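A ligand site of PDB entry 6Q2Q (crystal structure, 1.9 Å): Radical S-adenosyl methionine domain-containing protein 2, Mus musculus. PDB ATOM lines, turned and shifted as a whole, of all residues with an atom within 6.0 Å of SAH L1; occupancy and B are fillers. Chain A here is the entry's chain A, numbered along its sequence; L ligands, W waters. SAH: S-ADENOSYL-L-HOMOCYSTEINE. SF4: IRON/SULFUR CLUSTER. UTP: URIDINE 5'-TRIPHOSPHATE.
OXT of SAH L1 sits at hydrogen-bond distance from OG of Ser 136, at 2.4 Å. The guanidinium group of Arg 150 sits at hydrogen-bond distance from an oxygen (O2') of SAH L1 (2.7 Å). The backbone carbonyl oxygen (O) of Gly 82 sits close to a nitrogen (N) of SAH L1. O of Phe 46 sits at hydrogen-bond distance from N6 of SAH L1 (2.8 Å). N of Leu 208 is in hydrogen-bond range of N1 of SAH L1 (2.9 Å). The backbone carbonyl oxygen of Leu 208 sits at hydrogen-bond distance from a nitrogen (N6) of SAH L1 (3.0 Å). N of Phe 48 is in hydrogen-bond range of N7 of SAH L1 (3.3 Å). The side-chain amide nitrogen (ND2) of Asn 178 sits at hydrogen-bond distance from an oxygen (O3') of SAH L1 (3.3 Å). The side-chain carboxylate of Glu 83 lies close to a nitrogen (N) of SAH L1 (3.4 Å). A nitrogen (N6) of SAH L1 lies close to the side-chain amide nitrogen (ND2) of Asn 214, 3.4 Å away. NH1 of Arg 150 lies close to S3 of SF4 L2, at 3.4 Å. The backbone NH of Gly 82 lies close to a sulfur (S2) of SF4 L2 (3.6 Å). The side-chain amide nitrogen (ND2) of Asn 114 sits close to a sulfur (S3) of SF4 L2, 3.5 Å away. The side-chain sulfur (SG) of Cys 47 binds an iron atom (FE3) of SF4 L2. SG of Cys 40 is bound to FE1 of SF4 L2 (2.3 Å). A sulfur (S4) of SF4 L2 lies close to the backbone NH (N) of Cys 44. The side-chain sulfur of Cys 44 binds an iron atom (FE2) of SF4 L2, at 2.4 Å. An oxygen (O2A) of UTP L3 lies within hydrogen-bond range of the side-chain amide nitrogen (ND2) of Asn 178, 2.9 Å away. The side-chain hydroxyl (OG) of Ser 80 lies within hydrogen-bond range of an oxygen (O3') of UTP L3 (3.2 Å). An oxygen (O2') of UTP L3 sits at hydrogen-bond distance from a ring nitrogen (NE2) of His 35 (2.9 Å).
The backbone carbonyl oxygen (O) of Ser 113 sits close to an oxygen (OXT) of SAH L1. CA of Cys 47 touches N7 of SAH L1, at 3.7 Å. OG of Ser 80 touches CB of SAH L1, at 3.6 Å. Gly 81 touches SAH L1. Val 112 touches SAH L1. Asn 114 touches SAH L1. Val 180 touches SAH L1. Phe 205 touches SAH L1. O of Gln 206 touches C2 of SAH L1 (3.8 Å). Cys 207 touches SAH L1. Met 254 touches SAH L1. 20 residues have an atom within 4 Å of SAH L1: Phe 46, Cys 47, Phe 48, Ser 80, Gly 81, Gly 82, Glu 83, Val 112, Ser 113, Asn 114, Ser 136, Arg 150, Asn 178, Val 180, Phe 205, Gln 206, Cys 207, Leu 208, Asn 214 and Met 254.
Water W1 lies within hydrogen-bond range of OD1 of Asp 138, O2' of SAH L1, O of Asn 178, NH2 of Arg 150 and N of Val 180.
An oxygen (O) of SAH L1 binds an iron atom (FE4) of SF4 L2.
The side-chain sulfur of Cys 44 sits close to the guanidinium group of Arg 150. The backbone carbonyl oxygen (O) of Phe 46 sits at hydrogen-bond distance from the side-chain amide nitrogen (ND2) of Asn 214, 2.9 Å away. The side-chain amide nitrogen of Asn 214 lies within hydrogen-bond range of the backbone carbonyl oxygen of Leu 208 (2.9 Å). OE2 of Glu 83 lies within hydrogen-bond range of OG of Ser 113 (2.7 Å). The side-chain carboxylate (OE1) of Glu 83 lies within hydrogen-bond range of the backbone NH (N) of Asn 114 (2.7 Å). The backbone carbonyl oxygen (O) of Gly 81 sits at hydrogen-bond distance from a ring nitrogen (ND1) of His 35 (2.7 Å). The side-chain sulfur (SG) of Cys 47 lies close to the backbone NH (N) of His 49 (3.5 Å). N of Phe 205 lies within hydrogen-bond range of O of Ser 179, 2.8 Å away.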
ATOM      1  N   HIS A  35      11.662 -14.429  20.483  1.00  0.00           N
ATOM      2  CA  HIS A  35      10.269 -14.036  20.242  1.00  0.00           C
ATOM      3  C   HIS A  35       9.776 -13.337  21.511  1.00  0.00           C
ATOM      4  O   HIS A  35       9.197 -13.959  22.400  1.00  0.00           O
ATOM      5  CB  HIS A  35       9.433 -15.262  19.918  1.00  0.00           C
ATOM      6  CG  HIS A  35       9.816 -15.945  18.646  1.00  0.00           C
ATOM      7  ND1 HIS A  35       8.987 -15.989  17.543  1.00  0.00           N
ATOM      8  CD2 HIS A  35      10.933 -16.651  18.301  1.00  0.00           C
ATOM      9  CE1 HIS A  35       9.566 -16.691  16.581  1.00  0.00           C
ATOM     10  NE2 HIS A  35      10.755 -17.088  17.006  1.00  0.00           N
ATOM     11  N   CYS A  40       0.180  -9.883  18.088  1.00  0.00           N
ATOM     12  CA  CYS A  40       0.321  -9.580  16.661  1.00  0.00           C
ATOM     13  C   CYS A  40      -0.928  -8.863  16.178  1.00  0.00           C
ATOM     14  O   CYS A  40      -1.986  -8.983  16.774  1.00  0.00           O
ATOM     15  CB  CYS A  40       0.549 -10.840  15.817  1.00  0.00           C
ATOM     16  SG  CYS A  40       0.939 -10.360  14.107  1.00  0.00           S
ATOM     17  N   CYS A  44      -2.643 -14.345  10.106  1.00  0.00           N
ATOM     18  CA  CYS A  44      -2.283 -15.375   9.136  1.00  0.00           C
ATOM     19  C   CYS A  44      -2.793 -16.723   9.610  1.00  0.00           C
ATOM     20  O   CYS A  44      -2.565 -17.126  10.753  1.00  0.00           O
ATOM     21  CB  CYS A  44      -0.765 -15.405   8.968  1.00  0.00           C
ATOM     22  SG  CYS A  44      -0.069 -13.762   8.708  1.00  0.00           S
ATOM     23  N   PHE A  46      -2.034 -19.778   9.089  1.00  0.00           N
ATOM     24  CA  PHE A  46      -1.092 -20.848   9.426  1.00  0.00           C
ATOM     25  C   PHE A  46      -0.177 -20.506  10.598  1.00  0.00           C
ATOM     26  O   PHE A  46       0.703 -21.321  10.926  1.00  0.00           O
ATOM     27  CB  PHE A  46      -0.237 -21.200   8.210  1.00  0.00           C
ATOM     28  CG  PHE A  46       0.389 -20.003   7.546  1.00  0.00           C
ATOM     29  CD1 PHE A  46       1.337 -19.228   8.219  1.00  0.00           C
ATOM     30  CD2 PHE A  46       0.020 -19.639   6.259  1.00  0.00           C
ATOM     31  CE1 PHE A  46       1.912 -18.094   7.618  1.00  0.00           C
ATOM     32  CE2 PHE A  46       0.595 -18.522   5.653  1.00  0.00           C
ATOM     33  CZ  PHE A  46       1.529 -17.748   6.328  1.00  0.00           C
ATOM     34  N   CYS A  47      -0.322 -19.320  11.210  1.00  0.00           N
ATOM     35  CA  CYS A  47       0.679 -18.808  12.146  1.00  0.00           C
ATOM     36  C   CYS A  47       1.129 -19.864  13.168  1.00  0.00           C
ATOM     37  O   CYS A  47       0.312 -20.448  13.871  1.00  0.00           O
ATOM     38  CB  CYS A  47       0.117 -17.595  12.882  1.00  0.00           C
ATOM     39  SG  CYS A  47       1.275 -16.908  14.045  1.00  0.00           S
ATOM     40  N   PHE A  48       2.440 -20.122  13.234  1.00  0.00           N
ATOM     41  CA  PHE A  48       2.931 -21.111  14.182  1.00  0.00           C
ATOM     42  C   PHE A  48       3.542 -20.484  15.448  1.00  0.00           C
ATOM     43  O   PHE A  48       4.184 -21.209  16.224  1.00  0.00           O
ATOM     44  CB  PHE A  48       3.914 -22.118  13.513  1.00  0.00           C
ATOM     45  CG  PHE A  48       5.216 -21.541  12.978  1.00  0.00           C
ATOM     46  CD1 PHE A  48       6.063 -22.366  12.233  1.00  0.00           C
ATOM     47  CD2 PHE A  48       5.611 -20.220  13.195  1.00  0.00           C
ATOM     48  CE1 PHE A  48       7.268 -21.920  11.729  1.00  0.00           C
ATOM     49  CE2 PHE A  48       6.848 -19.744  12.674  1.00  0.00           C
ATOM     50  CZ  PHE A  48       7.661 -20.591  11.940  1.00  0.00           C
ATOM     51  N   HIS A  49       3.331 -19.184  15.695  1.00  0.00           N
ATOM     52  CA  HIS A  49       3.768 -18.556  16.951  1.00  0.00           C
ATOM     53  C   HIS A  49       2.686 -17.562  17.398  1.00  0.00           C
ATOM     54  O   HIS A  49       2.782 -16.350  17.184  1.00  0.00           O
ATOM     55  CB  HIS A  49       5.139 -17.885  16.813  1.00  0.00           C
ATOM     56  CG  HIS A  49       5.842 -17.731  18.120  1.00  0.00           C
ATOM     57  ND1 HIS A  49       6.701 -18.694  18.613  1.00  0.00           N
ATOM     58  CD2 HIS A  49       5.755 -16.779  19.070  1.00  0.00           C
ATOM     59  CE1 HIS A  49       7.142 -18.315  19.795  1.00  0.00           C
ATOM     60  NE2 HIS A  49       6.594 -17.148  20.094  1.00  0.00           N
ATOM     61  N   SER A  80      11.854 -11.464  16.949  1.00  0.00           N
ATOM     62  CA  SER A  80      10.688 -12.015  16.278  1.00  0.00           C
ATOM     63  C   SER A  80       9.520 -11.975  17.250  1.00  0.00           C
ATOM     64  O   SER A  80       9.583 -11.351  18.312  1.00  0.00           O
ATOM     65  CB  SER A  80      11.012 -13.433  15.765  1.00  0.00           C
ATOM     66  OG  SER A  80      10.003 -13.905  14.870  1.00  0.00           O
ATOM     67  N   GLY A  81       8.437 -12.656  16.883  1.00  0.00           N
ATOM     68  CA  GLY A  81       7.259 -12.728  17.735  1.00  0.00           C
ATOM     69  C   GLY A  81       6.270 -13.724  17.178  1.00  0.00           C
ATOM     70  O   GLY A  81       6.693 -14.795  16.731  1.00  0.00           O
ATOM     71  N   GLY A  82       4.980 -13.399  17.166  1.00  0.00           N
ATOM     72  CA  GLY A  82       4.452 -12.077  17.454  1.00  0.00           C
ATOM     73  C   GLY A  82       4.909 -11.088  16.412  1.00  0.00           C
ATOM     74  O   GLY A  82       5.694 -11.434  15.520  1.00  0.00           O
ATOM     75  N   GLU A  83       4.459  -9.841  16.522  1.00  0.00           N
ATOM     76  CA  GLU A  83       4.958  -8.776  15.648  1.00  0.00           C
ATOM     77  C   GLU A  83       5.869  -7.872  16.462  1.00  0.00           C
ATOM     78  O   GLU A  83       5.372  -7.126  17.326  1.00  0.00           O
ATOM     79  CB  GLU A  83       3.810  -7.974  15.035  1.00  0.00           C
ATOM     80  CG  GLU A  83       4.269  -6.740  14.219  1.00  0.00           C
ATOM     81  CD  GLU A  83       5.469  -7.027  13.326  1.00  0.00           C
ATOM     82  OE1 GLU A  83       5.446  -8.076  12.649  1.00  0.00           O
ATOM     83  OE2 GLU A  83       6.427  -6.214  13.280  1.00  0.00           O
ATOM     84  N   PRO A  84       7.186  -7.915  16.254  1.00  0.00           N
ATOM     85  CA  PRO A  84       8.096  -7.251  17.200  1.00  0.00           C
ATOM     86  C   PRO A  84       7.937  -5.738  17.229  1.00  0.00           C
ATOM     87  O   PRO A  84       8.261  -5.140  18.260  1.00  0.00           O
ATOM     88  CB  PRO A  84       9.492  -7.676  16.712  1.00  0.00           C
ATOM     89  CG  PRO A  84       9.317  -8.219  15.336  1.00  0.00           C
ATOM     90  CD  PRO A  84       7.905  -8.734  15.250  1.00  0.00           C
ATOM     91  N   VAL A 112      12.699 -10.216  12.116  1.00  0.00           N
ATOM     92  CA  VAL A 112      11.672 -10.705  11.202  1.00  0.00           C
ATOM     93  C   VAL A 112      10.359 -10.016  11.571  1.00  0.00           C
ATOM     94  O   VAL A 112       9.929 -10.087  12.732  1.00  0.00           O
ATOM     95  CB  VAL A 112      11.547 -12.238  11.266  1.00  0.00           C
ATOM     96  CG1 VAL A 112      10.538 -12.731  10.254  1.00  0.00           C
ATOM     97  CG2 VAL A 112      12.879 -12.857  10.974  1.00  0.00           C
ATOM     98  N   SER A 113       9.727  -9.331  10.611  1.00  0.00           N
ATOM     99  CA  SER A 113       8.563  -8.497  10.887  1.00  0.00           C
ATOM    100  C   SER A 113       7.546  -8.615   9.761  1.00  0.00           C
ATOM    101  O   SER A 113       7.903  -8.849   8.605  1.00  0.00           O
ATOM    102  CB  SER A 113       8.956  -7.013  11.055  1.00  0.00           C
ATOM    103  OG  SER A 113       7.788  -6.185  10.956  1.00  0.00           O
ATOM    104  N   ASN A 114       6.271  -8.390  10.076  1.00  0.00           N
ATOM    105  CA  ASN A 114       5.293  -8.354   8.999  1.00  0.00           C
ATOM    106  C   ASN A 114       5.294  -7.021   8.261  1.00  0.00           C
ATOM    107  O   ASN A 114       4.573  -6.892   7.272  1.00  0.00           O
ATOM    108  CB  ASN A 114       3.884  -8.703   9.516  1.00  0.00           C
ATOM    109  CG  ASN A 114       3.310  -7.653  10.461  1.00  0.00           C
ATOM    110  OD1 ASN A 114       3.667  -6.469  10.405  1.00  0.00           O
ATOM    111  ND2 ASN A 114       2.361  -8.074  11.305  1.00  0.00           N
ATOM    112  N   ALA A 134      14.210  -8.484   7.842  1.00  0.00           N
ATOM    113  CA  ALA A 134      13.414  -9.420   7.060  1.00  0.00           C
ATOM    114  C   ALA A 134      11.942  -9.017   7.133  1.00  0.00           C
ATOM    115  O   ALA A 134      11.395  -8.836   8.225  1.00  0.00           O
ATOM    116  CB  ALA A 134      13.588 -10.853   7.561  1.00  0.00           C
ATOM    117  N   ILE A 135      11.298  -8.881   5.977  1.00  0.00           N
ATOM    118  CA  ILE A 135       9.854  -8.657   5.929  1.00  0.00           C
ATOM    119  C   ILE A 135       9.197  -9.926   5.396  1.00  0.00           C
ATOM    120  O   ILE A 135       9.651 -10.466   4.379  1.00  0.00           O
ATOM    121  CB  ILE A 135       9.476  -7.447   5.057  1.00  0.00           C
ATOM    122  CG1 ILE A 135      10.236  -6.199   5.519  1.00  0.00           C
ATOM    123  CG2 ILE A 135       7.951  -7.242   5.108  1.00  0.00           C
ATOM    124  CD1 ILE A 135       9.925  -5.790   6.963  1.00  0.00           C
ATOM    125  N   SER A 136       8.127 -10.369   6.045  1.00  0.00           N
ATOM    126  CA  SER A 136       7.402 -11.542   5.559  1.00  0.00           C
ATOM    127  C   SER A 136       6.464 -11.125   4.435  1.00  0.00           C
ATOM    128  O   SER A 136       5.677 -10.185   4.593  1.00  0.00           O
ATOM    129  CB  SER A 136       6.624 -12.205   6.685  1.00  0.00           C
ATOM    130  OG  SER A 136       7.543 -12.762   7.596  1.00  0.00           O
ATOM    131  N   ASP A 138       4.149 -13.327   1.618  1.00  0.00           N
ATOM    132  CA  ASP A 138       3.762 -14.640   1.130  1.00  0.00           C
ATOM    133  C   ASP A 138       3.176 -14.609  -0.277  1.00  0.00           C
ATOM    134  O   ASP A 138       3.111 -15.644  -0.940  1.00  0.00           O
ATOM    135  CB  ASP A 138       2.739 -15.277   2.072  1.00  0.00           C
ATOM    136  CG  ASP A 138       3.274 -15.449   3.484  1.00  0.00           C
ATOM    137  OD1 ASP A 138       4.502 -15.678   3.647  1.00  0.00           O
ATOM    138  OD2 ASP A 138       2.460 -15.337   4.437  1.00  0.00           O
ATOM    139  N   ARG A 150      -2.986 -11.903   5.890  1.00  0.00           N
ATOM    140  CA  ARG A 150      -1.918 -10.925   6.051  1.00  0.00           C
ATOM    141  C   ARG A 150      -2.506  -9.533   5.874  1.00  0.00           C
ATOM    142  O   ARG A 150      -2.579  -9.005   4.783  1.00  0.00           O
ATOM    143  CB  ARG A 150      -0.800 -11.135   5.043  1.00  0.00           C
ATOM    144  CG  ARG A 150       0.080 -12.281   5.340  1.00  0.00           C
ATOM    145  CD  ARG A 150       1.470 -11.884   5.860  1.00  0.00           C
ATOM    146  NE  ARG A 150       2.223 -13.135   5.988  1.00  0.00           N
ATOM    147  CZ  ARG A 150       3.090 -13.413   6.958  1.00  0.00           C
ATOM    148  NH1 ARG A 150       3.357 -12.532   7.897  1.00  0.00           N
ATOM    149  NH2 ARG A 150       3.684 -14.593   6.980  1.00  0.00           N
ATOM    150  N   ASN A 178      10.977 -13.117   3.713  1.00  0.00           N
ATOM    151  CA  ASN A 178      10.582 -14.460   4.113  1.00  0.00           C
ATOM    152  C   ASN A 178       9.239 -14.773   3.472  1.00  0.00           C
ATOM    153  O   ASN A 178       8.330 -13.950   3.531  1.00  0.00           O
ATOM    154  CB  ASN A 178      10.434 -14.587   5.651  1.00  0.00           C
ATOM    155  CG  ASN A 178      11.777 -14.584   6.378  1.00  0.00           C
ATOM    156  OD1 ASN A 178      12.813 -14.383   5.761  1.00  0.00           O
ATOM    157  ND2 ASN A 178      11.752 -14.813   7.706  1.00  0.00           N
ATOM    158  N   SER A 179       9.092 -15.975   2.874  1.00  0.00           N
ATOM    159  CA  SER A 179       7.803 -16.388   2.306  1.00  0.00           C
ATOM    160  C   SER A 179       7.437 -17.774   2.813  1.00  0.00           C
ATOM    161  O   SER A 179       8.274 -18.691   2.816  1.00  0.00           O
ATOM    162  CB  SER A 179       7.850 -16.400   0.771  1.00  0.00           C
ATOM    163  OG  SER A 179       8.185 -15.117   0.266  1.00  0.00           O
ATOM    164  N   VAL A 180       6.183 -17.941   3.234  1.00  0.00           N
ATOM    165  CA  VAL A 180       5.635 -19.238   3.633  1.00  0.00           C
ATOM    166  C   VAL A 180       4.878 -19.806   2.452  1.00  0.00           C
ATOM    167  O   VAL A 180       3.892 -19.204   2.005  1.00  0.00           O
ATOM    168  CB  VAL A 180       4.712 -19.113   4.858  1.00  0.00           C
ATOM    169  CG1 VAL A 180       4.152 -20.517   5.248  1.00  0.00           C
ATOM    170  CG2 VAL A 180       5.436 -18.465   6.038  1.00  0.00           C
ATOM    171  N   PHE A 205       9.938 -20.944   3.087  1.00  0.00           N
ATOM    172  CA  PHE A 205       9.581 -21.948   4.080  1.00  0.00           C
ATOM    173  C   PHE A 205       8.398 -22.761   3.569  1.00  0.00           C
ATOM    174  O   PHE A 205       7.400 -22.192   3.130  1.00  0.00           O
ATOM    175  CB  PHE A 205       9.157 -21.332   5.426  1.00  0.00           C
ATOM    176  CG  PHE A 205      10.082 -20.301   5.994  1.00  0.00           C
ATOM    177  CD1 PHE A 205      11.409 -20.595   6.252  1.00  0.00           C
ATOM    178  CD2 PHE A 205       9.601 -19.050   6.362  1.00  0.00           C
ATOM    179  CE1 PHE A 205      12.258 -19.629   6.818  1.00  0.00           C
ATOM    180  CE2 PHE A 205      10.428 -18.089   6.926  1.00  0.00           C
ATOM    181  CZ  PHE A 205      11.752 -18.383   7.167  1.00  0.00           C
ATOM    182  N   GLN A 206       8.484 -24.076   3.697  1.00  0.00           N
ATOM    183  CA  GLN A 206       7.274 -24.885   3.548  1.00  0.00           C
ATOM    184  C   GLN A 206       6.383 -24.657   4.773  1.00  0.00           C
ATOM    185  O   GLN A 206       6.871 -24.644   5.898  1.00  0.00           O
ATOM    186  CB  GLN A 206       7.631 -26.365   3.429  1.00  0.00           C
ATOM    187  CG  GLN A 206       6.422 -27.276   3.223  1.00  0.00           C
ATOM    188  CD  GLN A 206       6.815 -28.730   3.150  1.00  0.00           C
ATOM    189  OE1 GLN A 206       7.971 -29.081   3.404  1.00  0.00           O
ATOM    190  NE2 GLN A 206       5.841 -29.599   2.823  1.00  0.00           N
ATOM    191  N   CYS A 207       5.089 -24.439   4.557  1.00  0.00           N
ATOM    192  CA  CYS A 207       4.193 -24.264   5.707  1.00  0.00           C
ATOM    193  C   CYS A 207       4.367 -25.414   6.698  1.00  0.00           C
ATOM    194  O   CYS A 207       4.361 -26.584   6.320  1.00  0.00           O
ATOM    195  CB  CYS A 207       2.730 -24.186   5.248  1.00  0.00           C
ATOM    196  SG  CYS A 207       1.591 -23.641   6.527  1.00  0.00           S
ATOM    197  N   LEU A 208       4.520 -25.083   7.987  1.00  0.00           N
ATOM    198  CA  LEU A 208       4.886 -26.057   9.006  1.00  0.00           C
ATOM    199  C   LEU A 208       3.807 -26.173  10.069  1.00  0.00           C
ATOM    200  O   LEU A 208       3.337 -25.165  10.597  1.00  0.00           O
ATOM    201  CB  LEU A 208       6.221 -25.666   9.653  1.00  0.00           C
ATOM    202  CG  LEU A 208       6.750 -26.612  10.741  1.00  0.00           C
ATOM    203  CD1 LEU A 208       7.107 -27.984  10.145  1.00  0.00           C
ATOM    204  CD2 LEU A 208       7.945 -25.978  11.434  1.00  0.00           C
ATOM    205  N   LEU A 209       3.431 -27.397  10.406  1.00  0.00           N
ATOM    206  CA  LEU A 209       2.430 -27.677  11.427  1.00  0.00           C
ATOM    207  C   LEU A 209       3.105 -27.814  12.784  1.00  0.00           C
ATOM    208  O   LEU A 209       4.063 -28.586  12.927  1.00  0.00           O
ATOM    209  CB  LEU A 209       1.697 -28.976  11.061  1.00  0.00           C
ATOM    210  CG  LEU A 209       0.261 -29.232  11.488  1.00  0.00           C
ATOM    211  CD1 LEU A 209      -0.660 -28.146  10.958  1.00  0.00           C
ATOM    212  CD2 LEU A 209      -0.173 -30.609  11.009  1.00  0.00           C
ATOM    213  N   ASN A 214      -0.690 -24.141  15.749  1.00  0.00           N
ATOM    214  CA  ASN A 214      -1.604 -24.160  14.615  1.00  0.00           C
ATOM    215  C   ASN A 214      -2.171 -25.558  14.348  1.00  0.00           C
ATOM    216  O   ASN A 214      -2.670 -25.833  13.258  1.00  0.00           O
ATOM    217  CB  ASN A 214      -0.893 -23.603  13.373  1.00  0.00           C
ATOM    218  CG  ASN A 214       0.326 -24.447  12.964  1.00  0.00           C
ATOM    219  OD1 ASN A 214       0.536 -25.543  13.496  1.00  0.00           O
ATOM    220  ND2 ASN A 214       1.111 -23.943  12.032  1.00  0.00           N
ATOM    221  N   ALA A 223      -3.758 -24.920  10.894  1.00  0.00           N
ATOM    222  CA  ALA A 223      -2.993 -24.798   9.653  1.00  0.00           C
ATOM    223  C   ALA A 223      -3.204 -25.942   8.678  1.00  0.00           C
ATOM    224  O   ALA A 223      -2.674 -25.863   7.558  1.00  0.00           O
ATOM    225  CB  ALA A 223      -1.500 -24.708   9.958  1.00  0.00           C
ATOM    226  N   MET A 254      13.437 -27.135   8.643  1.00  0.00           N
ATOM    227  CA  MET A 254      13.005 -26.055   9.509  1.00  0.00           C
ATOM    228  C   MET A 254      12.771 -26.477  10.948  1.00  0.00           C
ATOM    229  O   MET A 254      13.050 -25.685  11.862  1.00  0.00           O
ATOM    230  CB  MET A 254      11.728 -25.430   8.939  1.00  0.00           C
ATOM    231  CG  MET A 254      11.482 -24.016   9.408  1.00  0.00           C
ATOM    232  SD  MET A 254      10.003 -23.306   8.657  1.00  0.00           S
ATOM    233  CE  MET A 254      10.079 -21.670   9.399  1.00  0.00           C
HETATM  234  N   SAH L   1       5.187 -11.425  12.783  1.00  0.00           N
HETATM  235  CA  SAH L   1       6.503 -11.564  12.125  1.00  0.00           C
HETATM  236  CB  SAH L   1       7.393 -12.589  12.853  1.00  0.00           C
HETATM  237  CG  SAH L   1       6.602 -13.753  13.483  1.00  0.00           C
HETATM  238  SD  SAH L   1       6.551 -15.222  12.411  1.00  0.00           S
HETATM  239  C   SAH L   1       6.332 -11.981  10.682  1.00  0.00           C
HETATM  240  O   SAH L   1       5.287 -12.407  10.263  1.00  0.00           O
HETATM  241  OXT SAH L   1       7.349 -11.851   9.829  1.00  0.00           O
HETATM  242  C5' SAH L   1       8.308 -15.492  11.967  1.00  0.00           C
HETATM  243  C4' SAH L   1       8.397 -16.102  10.554  1.00  0.00           C
HETATM  244  O4' SAH L   1       7.754 -17.409  10.559  1.00  0.00           O
HETATM  245  C3' SAH L   1       7.679 -15.258   9.473  1.00  0.00           C
HETATM  246  O3' SAH L   1       8.487 -15.167   8.301  1.00  0.00           O
HETATM  247  C2' SAH L   1       6.392 -16.083   9.180  1.00  0.00           C
HETATM  248  O2' SAH L   1       5.922 -15.879   7.850  1.00  0.00           O
HETATM  249  C1' SAH L   1       6.918 -17.518   9.400  1.00  0.00           C
HETATM  250  N9  SAH L   1       5.828 -18.479   9.671  1.00  0.00           N
HETATM  251  C8  SAH L   1       4.677 -18.260  10.386  1.00  0.00           C
HETATM  252  N7  SAH L   1       3.961 -19.357  10.425  1.00  0.00           N
HETATM  253  C5  SAH L   1       4.632 -20.312   9.713  1.00  0.00           C
HETATM  254  C6  SAH L   1       4.358 -21.648   9.410  1.00  0.00           C
HETATM  255  N6  SAH L   1       3.173 -22.245   9.870  1.00  0.00           N
HETATM  256  N1  SAH L   1       5.258 -22.324   8.670  1.00  0.00           N
HETATM  257  C2  SAH L   1       6.377 -21.755   8.240  1.00  0.00           C
HETATM  258  N3  SAH L   1       6.682 -20.494   8.497  1.00  0.00           N
HETATM  259  C4  SAH L   1       5.831 -19.772   9.239  1.00  0.00           C
HETATM  260 FE1  SF4 L   2       1.446 -12.340  13.015  1.00  0.00          FE
HETATM  261 FE2  SF4 L   2       1.220 -13.597  10.693  1.00  0.00          FE
HETATM  262 FE3  SF4 L   2       1.828 -14.960  12.887  1.00  0.00          FE
HETATM  263 FE4  SF4 L   2       3.625 -13.073  11.829  1.00  0.00          FE
HETATM  264  S1  SF4 L   2       2.902 -15.085  10.888  1.00  0.00           S
HETATM  265  S2  SF4 L   2       3.044 -13.461  14.084  1.00  0.00           S
HETATM  266  S3  SF4 L   2       2.170 -11.565  10.958  1.00  0.00           S
HETATM  267  S4  SF4 L   2      -0.120 -13.942  12.548  1.00  0.00           S
HETATM  268  PA  UTP L   3      14.109 -16.785   9.766  1.00  0.00           P
HETATM  269  O1A UTP L   3      14.491 -18.164   9.066  1.00  0.00           O
HETATM  270  O2A UTP L   3      14.238 -15.622   8.859  1.00  0.00           O
HETATM  271  O3A UTP L   3      15.054 -16.584  11.027  1.00  0.00           O
HETATM  272  O5' UTP L   3      12.625 -16.837  10.369  1.00  0.00           O
HETATM  273  PB  UTP L   3      16.589 -16.171  11.133  1.00  0.00           P
HETATM  274  O1B UTP L   3      16.799 -14.707  11.124  1.00  0.00           O
HETATM  275  O2B UTP L   3      17.198 -16.847  12.443  1.00  0.00           O
HETATM  276  O3B UTP L   3      17.199 -16.852   9.842  1.00  0.00           O
HETATM  277  PG  UTP L   3      18.642 -16.703   9.192  1.00  0.00           P
HETATM  278  O1G UTP L   3      19.610 -16.335  10.266  1.00  0.00           O
HETATM  279  O2G UTP L   3      18.966 -18.094   8.491  1.00  0.00           O
HETATM  280  O3G UTP L   3      18.517 -15.585   8.075  1.00  0.00           O
HETATM  281  C5' UTP L   3      12.143 -18.078  10.866  1.00  0.00           C
HETATM  282  C4' UTP L   3      11.338 -17.732  12.115  1.00  0.00           C
HETATM  283  O4' UTP L   3      10.486 -18.842  12.432  1.00  0.00           O
HETATM  284  C1' UTP L   3      10.715 -19.194  13.820  1.00  0.00           C
HETATM  285  C2' UTP L   3      12.202 -18.872  14.035  1.00  0.00           C
HETATM  286  O2' UTP L   3      12.477 -18.753  15.433  1.00  0.00           O
HETATM  287  C3' UTP L   3      12.303 -17.527  13.290  1.00  0.00           C
HETATM  288  O3' UTP L   3      11.829 -16.453  14.123  1.00  0.00           O
HETATM  289  N1  UTP L   3      10.487 -20.638  13.932  1.00  0.00           N
HETATM  290  C6  UTP L   3      11.256 -21.486  13.190  1.00  0.00           C
HETATM  291  C2  UTP L   3       9.511 -21.089  14.740  1.00  0.00           C
HETATM  292  O2  UTP L   3       8.866 -20.277  15.366  1.00  0.00           O
HETATM  293  N3  UTP L   3       9.270 -22.415  14.847  1.00  0.00           N
HETATM  294  C4  UTP L   3      10.023 -23.284  14.131  1.00  0.00           C
HETATM  295  O4  UTP L   3       9.829 -24.486  14.210  1.00  0.00           O
HETATM  296  C5  UTP L   3      11.054 -22.819  13.278  1.00  0.00           C
HETATM  297  O   HOH W   1       6.411 -15.234   5.315  1.00  0.00           O
